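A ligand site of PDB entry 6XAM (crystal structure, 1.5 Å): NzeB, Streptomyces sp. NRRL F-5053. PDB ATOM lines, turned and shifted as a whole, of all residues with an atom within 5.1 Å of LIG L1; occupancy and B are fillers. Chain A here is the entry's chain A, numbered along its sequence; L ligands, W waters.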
ATOM      1  N   GLN A  75      27.835 -22.134 -30.988  1.00  0.00           N
ATOM      2  CA  GLN A  75      29.150 -22.714 -30.757  1.00  0.00           C
ATOM      3  C   GLN A  75      29.091 -24.019 -29.978  1.00  0.00           C
ATOM      4  O   GLN A  75      29.986 -24.853 -30.104  1.00  0.00           O
ATOM      5  CB  GLN A  75      30.058 -21.709 -30.029  1.00  0.00           C
ATOM      6  CG  GLN A  75      29.491 -21.240 -28.719  1.00  0.00           C
ATOM      7  CD  GLN A  75      30.064 -19.894 -28.230  1.00  0.00           C
ATOM      8  OE1 GLN A  75      31.253 -19.777 -27.887  1.00  0.00           O
ATOM      9  NE2 GLN A  75      29.198 -18.885 -28.160  1.00  0.00           N
ATOM     10  N   GLU A  76      28.054 -24.208 -29.151  1.00  0.00           N
ATOM     11  CA  GLU A  76      28.019 -25.366 -28.278  1.00  0.00           C
ATOM     12  C   GLU A  76      27.549 -26.601 -29.044  1.00  0.00           C
ATOM     13  O   GLU A  76      26.704 -26.502 -29.949  1.00  0.00           O
ATOM     14  CB  GLU A  76      27.117 -25.114 -27.080  1.00  0.00           C
ATOM     15  CG  GLU A  76      25.652 -24.882 -27.399  1.00  0.00           C
ATOM     16  CD  GLU A  76      25.293 -23.421 -27.644  1.00  0.00           C
ATOM     17  OE1 GLU A  76      24.093 -23.087 -27.571  1.00  0.00           O
ATOM     18  OE2 GLU A  76      26.206 -22.603 -27.910  1.00  0.00           O
ATOM     19  N   LEU A  80      21.495 -26.172 -25.280  1.00  0.00           N
ATOM     20  CA  LEU A  80      21.561 -26.134 -23.822  1.00  0.00           C
ATOM     21  C   LEU A  80      20.194 -26.176 -23.162  1.00  0.00           C
ATOM     22  O   LEU A  80      19.971 -25.552 -22.121  1.00  0.00           O
ATOM     23  CB  LEU A  80      22.340 -24.901 -23.368  1.00  0.00           C
ATOM     24  CG  LEU A  80      23.721 -24.745 -24.013  1.00  0.00           C
ATOM     25  CD1 LEU A  80      24.427 -23.497 -23.497  1.00  0.00           C
ATOM     26  CD2 LEU A  80      24.561 -25.995 -23.771  1.00  0.00           C
ATOM     27  N   PHE A 177      32.376 -28.447 -24.330  1.00  0.00           N
ATOM     28  CA  PHE A 177      32.588 -28.503 -25.767  1.00  0.00           C
ATOM     29  C   PHE A 177      32.979 -29.919 -26.227  1.00  0.00           C
ATOM     30  O   PHE A 177      32.798 -30.281 -27.398  1.00  0.00           O
ATOM     31  CB  PHE A 177      33.694 -27.539 -26.159  1.00  0.00           C
ATOM     32  CG  PHE A 177      33.266 -26.105 -26.208  1.00  0.00           C
ATOM     33  CD1 PHE A 177      32.377 -25.680 -27.183  1.00  0.00           C
ATOM     34  CD2 PHE A 177      33.750 -25.179 -25.303  1.00  0.00           C
ATOM     35  CE1 PHE A 177      31.975 -24.364 -27.246  1.00  0.00           C
ATOM     36  CE2 PHE A 177      33.359 -23.856 -25.361  1.00  0.00           C
ATOM     37  CZ  PHE A 177      32.470 -23.451 -26.344  1.00  0.00           C
ATOM     38  N   THR A 244      30.155 -21.217 -12.959  1.00  0.00           N
ATOM     39  CA  THR A 244      30.779 -19.900 -13.081  1.00  0.00           C
ATOM     40  C   THR A 244      31.466 -19.522 -11.773  1.00  0.00           C
ATOM     41  O   THR A 244      32.652 -19.194 -11.752  1.00  0.00           O
ATOM     42  CB  THR A 244      29.665 -18.907 -13.388  1.00  0.00           C
ATOM     43  OG1 THR A 244      28.583 -19.131 -12.470  1.00  0.00           O
ATOM     44  CG2 THR A 244      29.167 -19.103 -14.828  1.00  0.00           C
ATOM     45  N   LEU A 286      37.706 -17.043 -17.698  1.00  0.00           N
ATOM     46  CA  LEU A 286      36.658 -17.956 -17.234  1.00  0.00           C
ATOM     47  C   LEU A 286      36.113 -18.820 -18.371  1.00  0.00           C
ATOM     48  O   LEU A 286      36.493 -19.980 -18.507  1.00  0.00           O
ATOM     49  CB  LEU A 286      35.552 -17.232 -16.477  1.00  0.00           C
ATOM     50  CG  LEU A 286      34.516 -18.191 -15.888  1.00  0.00           C
ATOM     51  CD1 LEU A 286      35.162 -19.221 -14.944  1.00  0.00           C
ATOM     52  CD2 LEU A 286      33.418 -17.408 -15.188  1.00  0.00           C
ATOM     53  N   SER A 287      35.210 -18.268 -19.175  1.00  0.00           N
ATOM     54  CA  SER A 287      34.673 -19.040 -20.289  1.00  0.00           C
ATOM     55  C   SER A 287      35.733 -19.358 -21.342  1.00  0.00           C
ATOM     56  O   SER A 287      36.574 -18.521 -21.676  1.00  0.00           O
ATOM     57  CB  SER A 287      33.523 -18.297 -20.949  1.00  0.00           C
ATOM     58  OG  SER A 287      32.981 -19.064 -22.027  1.00  0.00           O
ATOM     59  N   THR A 288      35.681 -20.574 -21.885  1.00  0.00           N
ATOM     60  CA  THR A 288      36.467 -20.970 -23.049  1.00  0.00           C
ATOM     61  C   THR A 288      35.723 -20.727 -24.358  1.00  0.00           C
ATOM     62  O   THR A 288      36.262 -21.023 -25.431  1.00  0.00           O
ATOM     63  CB  THR A 288      36.845 -22.459 -22.958  1.00  0.00           C
ATOM     64  OG1 THR A 288      35.663 -23.271 -22.922  1.00  0.00           O
ATOM     65  CG2 THR A 288      37.661 -22.716 -21.709  1.00  0.00           C
ATOM     66  N   GLY A 289      34.488 -20.232 -24.297  1.00  0.00           N
ATOM     67  CA  GLY A 289      33.797 -19.750 -25.479  1.00  0.00           C
ATOM     68  C   GLY A 289      33.545 -18.259 -25.403  1.00  0.00           C
ATOM     69  O   GLY A 289      34.365 -17.516 -24.849  1.00  0.00           O
ATOM     70  N   SER A 290      32.455 -17.826 -26.024  1.00  0.00           N
ATOM     71  CA  SER A 290      32.145 -16.411 -26.107  1.00  0.00           C
ATOM     72  C   SER A 290      30.700 -16.074 -25.839  1.00  0.00           C
ATOM     73  O   SER A 290      29.811 -16.896 -25.955  1.00  0.00           O
ATOM     74  CB  SER A 290      32.419 -15.931 -27.544  1.00  0.00           C
ATOM     75  OG  SER A 290      33.776 -15.951 -27.897  1.00  0.00           O
ATOM     76  N   VAL A 291      30.497 -14.818 -25.491  1.00  0.00           N
ATOM     77  CA  VAL A 291      29.158 -14.269 -25.362  1.00  0.00           C
ATOM     78  C   VAL A 291      28.670 -14.116 -26.828  1.00  0.00           C
ATOM     79  O   VAL A 291      29.453 -13.778 -27.719  1.00  0.00           O
ATOM     80  CB  VAL A 291      29.227 -12.910 -24.638  1.00  0.00           C
ATOM     81  CG1 VAL A 291      28.103 -11.977 -25.039  1.00  0.00           C
ATOM     82  CG2 VAL A 291      29.289 -13.115 -23.129  1.00  0.00           C
ATOM     83  N   LYS A 292      27.404 -14.390 -27.085  1.00  0.00           N
ATOM     84  CA  LYS A 292      26.916 -14.305 -28.461  1.00  0.00           C
ATOM     85  C   LYS A 292      25.599 -13.565 -28.623  1.00  0.00           C
ATOM     86  O   LYS A 292      24.798 -13.521 -27.732  1.00  0.00           O
ATOM     87  CB  LYS A 292      26.861 -15.694 -29.102  1.00  0.00           C
ATOM     88  CG  LYS A 292      25.621 -16.480 -28.770  1.00  0.00           C
ATOM     89  CD  LYS A 292      25.682 -17.008 -27.356  1.00  0.00           C
ATOM     90  CE  LYS A 292      24.602 -18.043 -27.092  1.00  0.00           C
ATOM     91  NZ  LYS A 292      24.254 -18.074 -25.658  1.00  0.00           N
ATOM     92  N   LEU A 316      35.174 -12.622 -24.005  1.00  0.00           N
ATOM     93  CA  LEU A 316      35.441 -11.682 -22.916  1.00  0.00           C
ATOM     94  C   LEU A 316      36.913 -11.704 -22.521  1.00  0.00           C
ATOM     95  O   LEU A 316      37.487 -10.665 -22.170  1.00  0.00           O
ATOM     96  CB  LEU A 316      34.553 -11.997 -21.708  1.00  0.00           C
ATOM     97  CG  LEU A 316      33.057 -12.058 -22.038  1.00  0.00           C
ATOM     98  CD1 LEU A 316      32.296 -12.331 -20.770  1.00  0.00           C
ATOM     99  CD2 LEU A 316      32.575 -10.761 -22.641  1.00  0.00           C
ATOM    100  N   GLY A 343      34.436  -8.839 -17.517  1.00  0.00           N
ATOM    101  CA  GLY A 343      34.247 -10.127 -16.853  1.00  0.00           C
ATOM    102  C   GLY A 343      32.792 -10.485 -16.590  1.00  0.00           C
ATOM    103  O   GLY A 343      32.452 -11.677 -16.473  1.00  0.00           O
ATOM    104  N   PHE A 390      32.942 -25.410 -20.577  1.00  0.00           N
ATOM    105  CA  PHE A 390      32.664 -24.010 -20.922  1.00  0.00           C
ATOM    106  C   PHE A 390      33.351 -23.066 -19.940  1.00  0.00           C
ATOM    107  O   PHE A 390      33.872 -22.015 -20.340  1.00  0.00           O
ATOM    108  CB  PHE A 390      31.165 -23.740 -20.848  1.00  0.00           C
ATOM    109  CG  PHE A 390      30.341 -24.398 -21.922  1.00  0.00           C
ATOM    110  CD1 PHE A 390      30.939 -24.994 -23.019  1.00  0.00           C
ATOM    111  CD2 PHE A 390      28.965 -24.389 -21.831  1.00  0.00           C
ATOM    112  CE1 PHE A 390      30.151 -25.582 -24.024  1.00  0.00           C
ATOM    113  CE2 PHE A 390      28.179 -24.992 -22.823  1.00  0.00           C
ATOM    114  CZ  PHE A 390      28.778 -25.581 -23.913  1.00  0.00           C
ATOM    115  N   PHE A 391      33.318 -23.397 -18.650  1.00  0.00           N
ATOM    116  CA  PHE A 391      33.838 -22.524 -17.601  1.00  0.00           C
ATOM    117  C   PHE A 391      35.049 -23.218 -16.978  1.00  0.00           C
ATOM    118  O   PHE A 391      34.905 -24.235 -16.285  1.00  0.00           O
ATOM    119  CB  PHE A 391      32.736 -22.171 -16.606  1.00  0.00           C
ATOM    120  CG  PHE A 391      31.563 -21.516 -17.265  1.00  0.00           C
ATOM    121  CD1 PHE A 391      31.688 -20.257 -17.826  1.00  0.00           C
ATOM    122  CD2 PHE A 391      30.355 -22.188 -17.399  1.00  0.00           C
ATOM    123  CE1 PHE A 391      30.621 -19.665 -18.489  1.00  0.00           C
ATOM    124  CE2 PHE A 391      29.265 -21.583 -18.073  1.00  0.00           C
ATOM    125  CZ  PHE A 391      29.406 -20.339 -18.608  1.00  0.00           C
HETATM  126  N1  LIG L   1      31.748 -15.731 -20.564  1.00  0.00           N
HETATM  127  C1  LIG L   1      27.460 -18.570 -23.417  1.00  0.00           C
HETATM  128  O1  LIG L   1      26.643 -17.830 -23.964  1.00  0.00           O
HETATM  129  C2  LIG L   1      28.328 -18.037 -22.311  1.00  0.00           C
HETATM  130  C3  LIG L   1      31.135 -16.043 -18.074  1.00  0.00           C
HETATM  131  C4  LIG L   1      28.455 -20.893 -23.210  1.00  0.00           C
HETATM  132  C5  LIG L   1      28.907 -21.963 -24.234  1.00  0.00           C
HETATM  133  C6  LIG L   1      29.862 -21.409 -25.288  1.00  0.00           C
HETATM  134  C7  LIG L   1      29.667 -20.154 -22.615  1.00  0.00           C
HETATM  135  C8  LIG L   1      28.646 -16.521 -22.415  1.00  0.00           C
HETATM  136  C9  LIG L   1      29.748 -16.217 -21.416  1.00  0.00           C
HETATM  137  C10 LIG L   1      31.040 -15.867 -21.755  1.00  0.00           C
HETATM  138  C11 LIG L   1      30.913 -16.017 -19.457  1.00  0.00           C
HETATM  139  C12 LIG L   1      29.618 -16.339 -19.997  1.00  0.00           C
HETATM  140  C13 LIG L   1      28.569 -16.680 -19.123  1.00  0.00           C
HETATM  141  C14 LIG L   1      28.787 -16.692 -17.754  1.00  0.00           C
HETATM  142  C15 LIG L   1      30.081 -16.390 -17.235  1.00  0.00           C
HETATM  143  N2  LIG L   1      29.577 -18.828 -22.219  1.00  0.00           N
HETATM  144  N3  LIG L   1      27.518 -19.911 -23.824  1.00  0.00           N
HETATM  145  O2  LIG L   1      30.757 -20.724 -22.457  1.00  0.00           O
HETATM  146  C1  LG2 L   2      25.066 -13.372 -17.191  1.00  0.00           C
HETATM  147  C2  LG2 L   2      29.646 -13.741 -15.594  1.00  0.00           C
HETATM  148  C3  LG2 L   2      28.043 -15.543 -11.400  1.00  0.00           C
HETATM  149  C4  LG2 L   2      23.487 -15.272 -13.017  1.00  0.00           C
HETATM  150  C5  LG2 L   2      26.432 -13.289 -17.105  1.00  0.00           C
HETATM  151  C6  LG2 L   2      27.301 -12.791 -18.154  1.00  0.00           C
HETATM  152  C7  LG2 L   2      28.557 -12.922 -17.693  1.00  0.00           C
HETATM  153  C8  LG2 L   2      28.536 -13.480 -16.368  1.00  0.00           C
HETATM  154  C9  LG2 L   2      29.834 -12.521 -18.436  1.00  0.00           C
HETATM  155  C10 LG2 L   2      26.867 -12.184 -19.515  1.00  0.00           C
HETATM  156  C11 LG2 L   2      26.528 -13.214 -20.582  1.00  0.00           C
HETATM  157  C12 LG2 L   2      26.072 -12.528 -21.851  1.00  0.00           C
HETATM  158  O1  LG2 L   2      26.316 -11.304 -22.046  1.00  0.00           O
HETATM  159  O2  LG2 L   2      25.458 -13.238 -22.701  1.00  0.00           O
HETATM  160  C13 LG2 L   2      29.614 -14.269 -14.324  1.00  0.00           C
HETATM  161  C14 LG2 L   2      30.765 -14.501 -13.470  1.00  0.00           C
HETATM  162  C15 LG2 L   2      30.299 -15.026 -12.319  1.00  0.00           C
HETATM  163  C16 LG2 L   2      28.869 -15.092 -12.416  1.00  0.00           C
HETATM  164  C17 LG2 L   2      32.222 -14.215 -13.886  1.00  0.00           C
HETATM  165  C18 LG2 L   2      31.070 -15.464 -11.062  1.00  0.00           C
HETATM  166  C19 LG2 L   2      32.347 -15.130 -10.833  1.00  0.00           C
HETATM  167  C20 LG2 L   2      26.671 -15.607 -11.449  1.00  0.00           C
HETATM  168  C21 LG2 L   2      25.812 -16.077 -10.386  1.00  0.00           C
HETATM  169  C22 LG2 L   2      24.542 -16.010 -10.840  1.00  0.00           C
HETATM  170  C23 LG2 L   2      24.564 -15.494 -12.180  1.00  0.00           C
HETATM  171  C24 LG2 L   2      26.293 -16.561  -8.992  1.00  0.00           C
HETATM  172  C25 LG2 L   2      23.309 -16.419 -10.011  1.00  0.00           C
HETATM  173  C26 LG2 L   2      22.265 -17.004 -10.626  1.00  0.00           C
HETATM  174  C27 LG2 L   2      23.530 -14.812 -14.320  1.00  0.00           C
HETATM  175  C28 LG2 L   2      22.421 -14.793 -15.266  1.00  0.00           C
HETATM  176  C29 LG2 L   2      22.847 -14.278 -16.418  1.00  0.00           C
HETATM  177  C30 LG2 L   2      24.248 -13.948 -16.252  1.00  0.00           C
HETATM  178  C31 LG2 L   2      21.005 -15.292 -14.955  1.00  0.00           C
HETATM  179  C32 LG2 L   2      22.020 -14.084 -17.702  1.00  0.00           C
HETATM  180  C33 LG2 L   2      21.681 -12.622 -17.950  1.00  0.00           C
HETATM  181  C34 LG2 L   2      21.092 -12.416 -19.321  1.00  0.00           C
HETATM  182  O3  LG2 L   2      21.357 -13.233 -20.252  1.00  0.00           O
HETATM  183  O4  LG2 L   2      20.360 -11.404 -19.443  1.00  0.00           O
HETATM  184  N1  LG2 L   2      27.215 -13.712 -16.028  1.00  0.00           N
HETATM  185  N2  LG2 L   2      28.455 -14.623 -13.648  1.00  0.00           N
HETATM  186  N3  LG2 L   2      25.883 -15.234 -12.519  1.00  0.00           N
HETATM  187  N4  LG2 L   2      24.650 -14.291 -14.971  1.00  0.00           N
HETATM  188 FE1  LG2 L   2      26.539 -14.236 -14.186  1.00  0.00          FE
HETATM  189  N1  LG3 L   3      25.251 -17.667 -18.212  1.00  0.00           N
HETATM  190  C1  LG3 L   3      22.433 -17.912 -22.539  1.00  0.00           C
HETATM  191  O1  LG3 L   3      22.991 -18.272 -23.580  1.00  0.00           O
HETATM  192  C2  LG3 L   3      22.706 -16.497 -21.980  1.00  0.00           C
HETATM  193  C3  LG3 L   3      25.838 -20.138 -18.562  1.00  0.00           C
HETATM  194  C4  LG3 L   3      20.861 -18.550 -20.641  1.00  0.00           C
HETATM  195  C5  LG3 L   3      21.373 -19.421 -19.436  1.00  0.00           C
HETATM  196  C6  LG3 L   3      22.169 -18.635 -18.411  1.00  0.00           C
HETATM  197  C7  LG3 L   3      20.880 -17.023 -20.305  1.00  0.00           C
HETATM  198  C8  LG3 L   3      24.217 -16.363 -21.515  1.00  0.00           C
HETATM  199  C9  LG3 L   3      24.671 -17.182 -20.328  1.00  0.00           C
HETATM  200  C10 LG3 L   3      24.802 -16.655 -19.072  1.00  0.00           C
HETATM  201  C11 LG3 L   3      25.421 -18.860 -18.947  1.00  0.00           C
HETATM  202  C12 LG3 L   3      25.051 -18.575 -20.313  1.00  0.00           C
HETATM  203  C13 LG3 L   3      25.136 -19.616 -21.266  1.00  0.00           C
HETATM  204  C14 LG3 L   3      25.562 -20.872 -20.875  1.00  0.00           C
HETATM  205  C15 LG3 L   3      25.916 -21.129 -19.534  1.00  0.00           C
HETATM  206  N2  LG3 L   3      21.733 -16.138 -20.933  1.00  0.00           N
HETATM  207  N3  LG3 L   3      21.589 -18.797 -21.913  1.00  0.00           N
HETATM  208  O2  LG3 L   3      20.125 -16.570 -19.445  1.00  0.00           O
HETATM  209  O   HOH W   1      26.290 -16.867 -15.514  1.00  0.00           O
HETATM  210  O   HOH W   2      34.328 -15.377 -19.362  1.00  0.00           O
HETATM  211  O   HOH W   3      25.498 -20.886 -25.589  1.00  0.00           O
HETATM  212  O   HOH W   4      34.115 -15.269 -23.119  1.00  0.00           O
HETATM  213  O   HOH W   5      26.010 -15.199 -24.504  1.00  0.00           O
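Water W5 lies within hydrogen-bond range of an oxygen (O2) of LG2 L2 (2.7 Å), an oxygen (O1) of LIG L1 (2.8 Å) and the backbone NH (N) of Lys 292 (3.0 Å).
Water W3 lies within hydrogen-bond range of N3 of LIG L1, OE2 of Glu 76 and NZ of Lys 292.
Water W2 lies within hydrogen-bond range of a nitrogen (N1) of LIG L1 (2.9 Å) and the backbone NH (N) of Ser 287 (3.0 Å).
Water W4 bridges O of Gly 289 (2.8 Å) and N of Leu 316 (3.0 Å).
The side-chain hydroxyl of Ser 287 sits at hydrogen-bond distance from the backbone NH of Gly 289, 3.0 Å away.
The backbone carbonyl oxygen (O) of Phe 390 is in hydrogen-bond range of the backbone NH (N) of Thr 288, 2.8 Å away.
OE1 of Gln 75 is in hydrogen-bond range of N of Ser 290 (3.0 Å).
The side-chain amino group (NZ) of Lys 292 is in hydrogen-bond range of an oxygen (O1) of LIG L1.
The side-chain hydroxyl (OG) of Ser 287 sits at hydrogen-bond distance from an oxygen (O2) of LIG L1.
O1 of LG3 L3 is in hydrogen-bond range of NZ of Lys 292, 2.4 Å away.
O3 of LG2 L2 sits at hydrogen-bond distance from N2 of LG3 L3.
Merely in contact with LIG L1: Gln 75 (3.3 Å), Phe 390 (3.4 Å), Leu 316 (3.5 Å), Phe 177 (3.5 Å), Val 291 (3.5 Å), Phe 391 (3.5 Å), Thr 244 (3.7 Å), Ser 290 (3.7 Å) and Leu 286 (3.9 Å).
Hydrophobic or aromatic side chains within 4 Å of LIG L1: Phe 177, Leu 286, Val 291, Leu 316, Phe 390 and Phe 391.
The nearest printed residue that does not touch LIG L1 is Gly 289 (4.2 Å).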
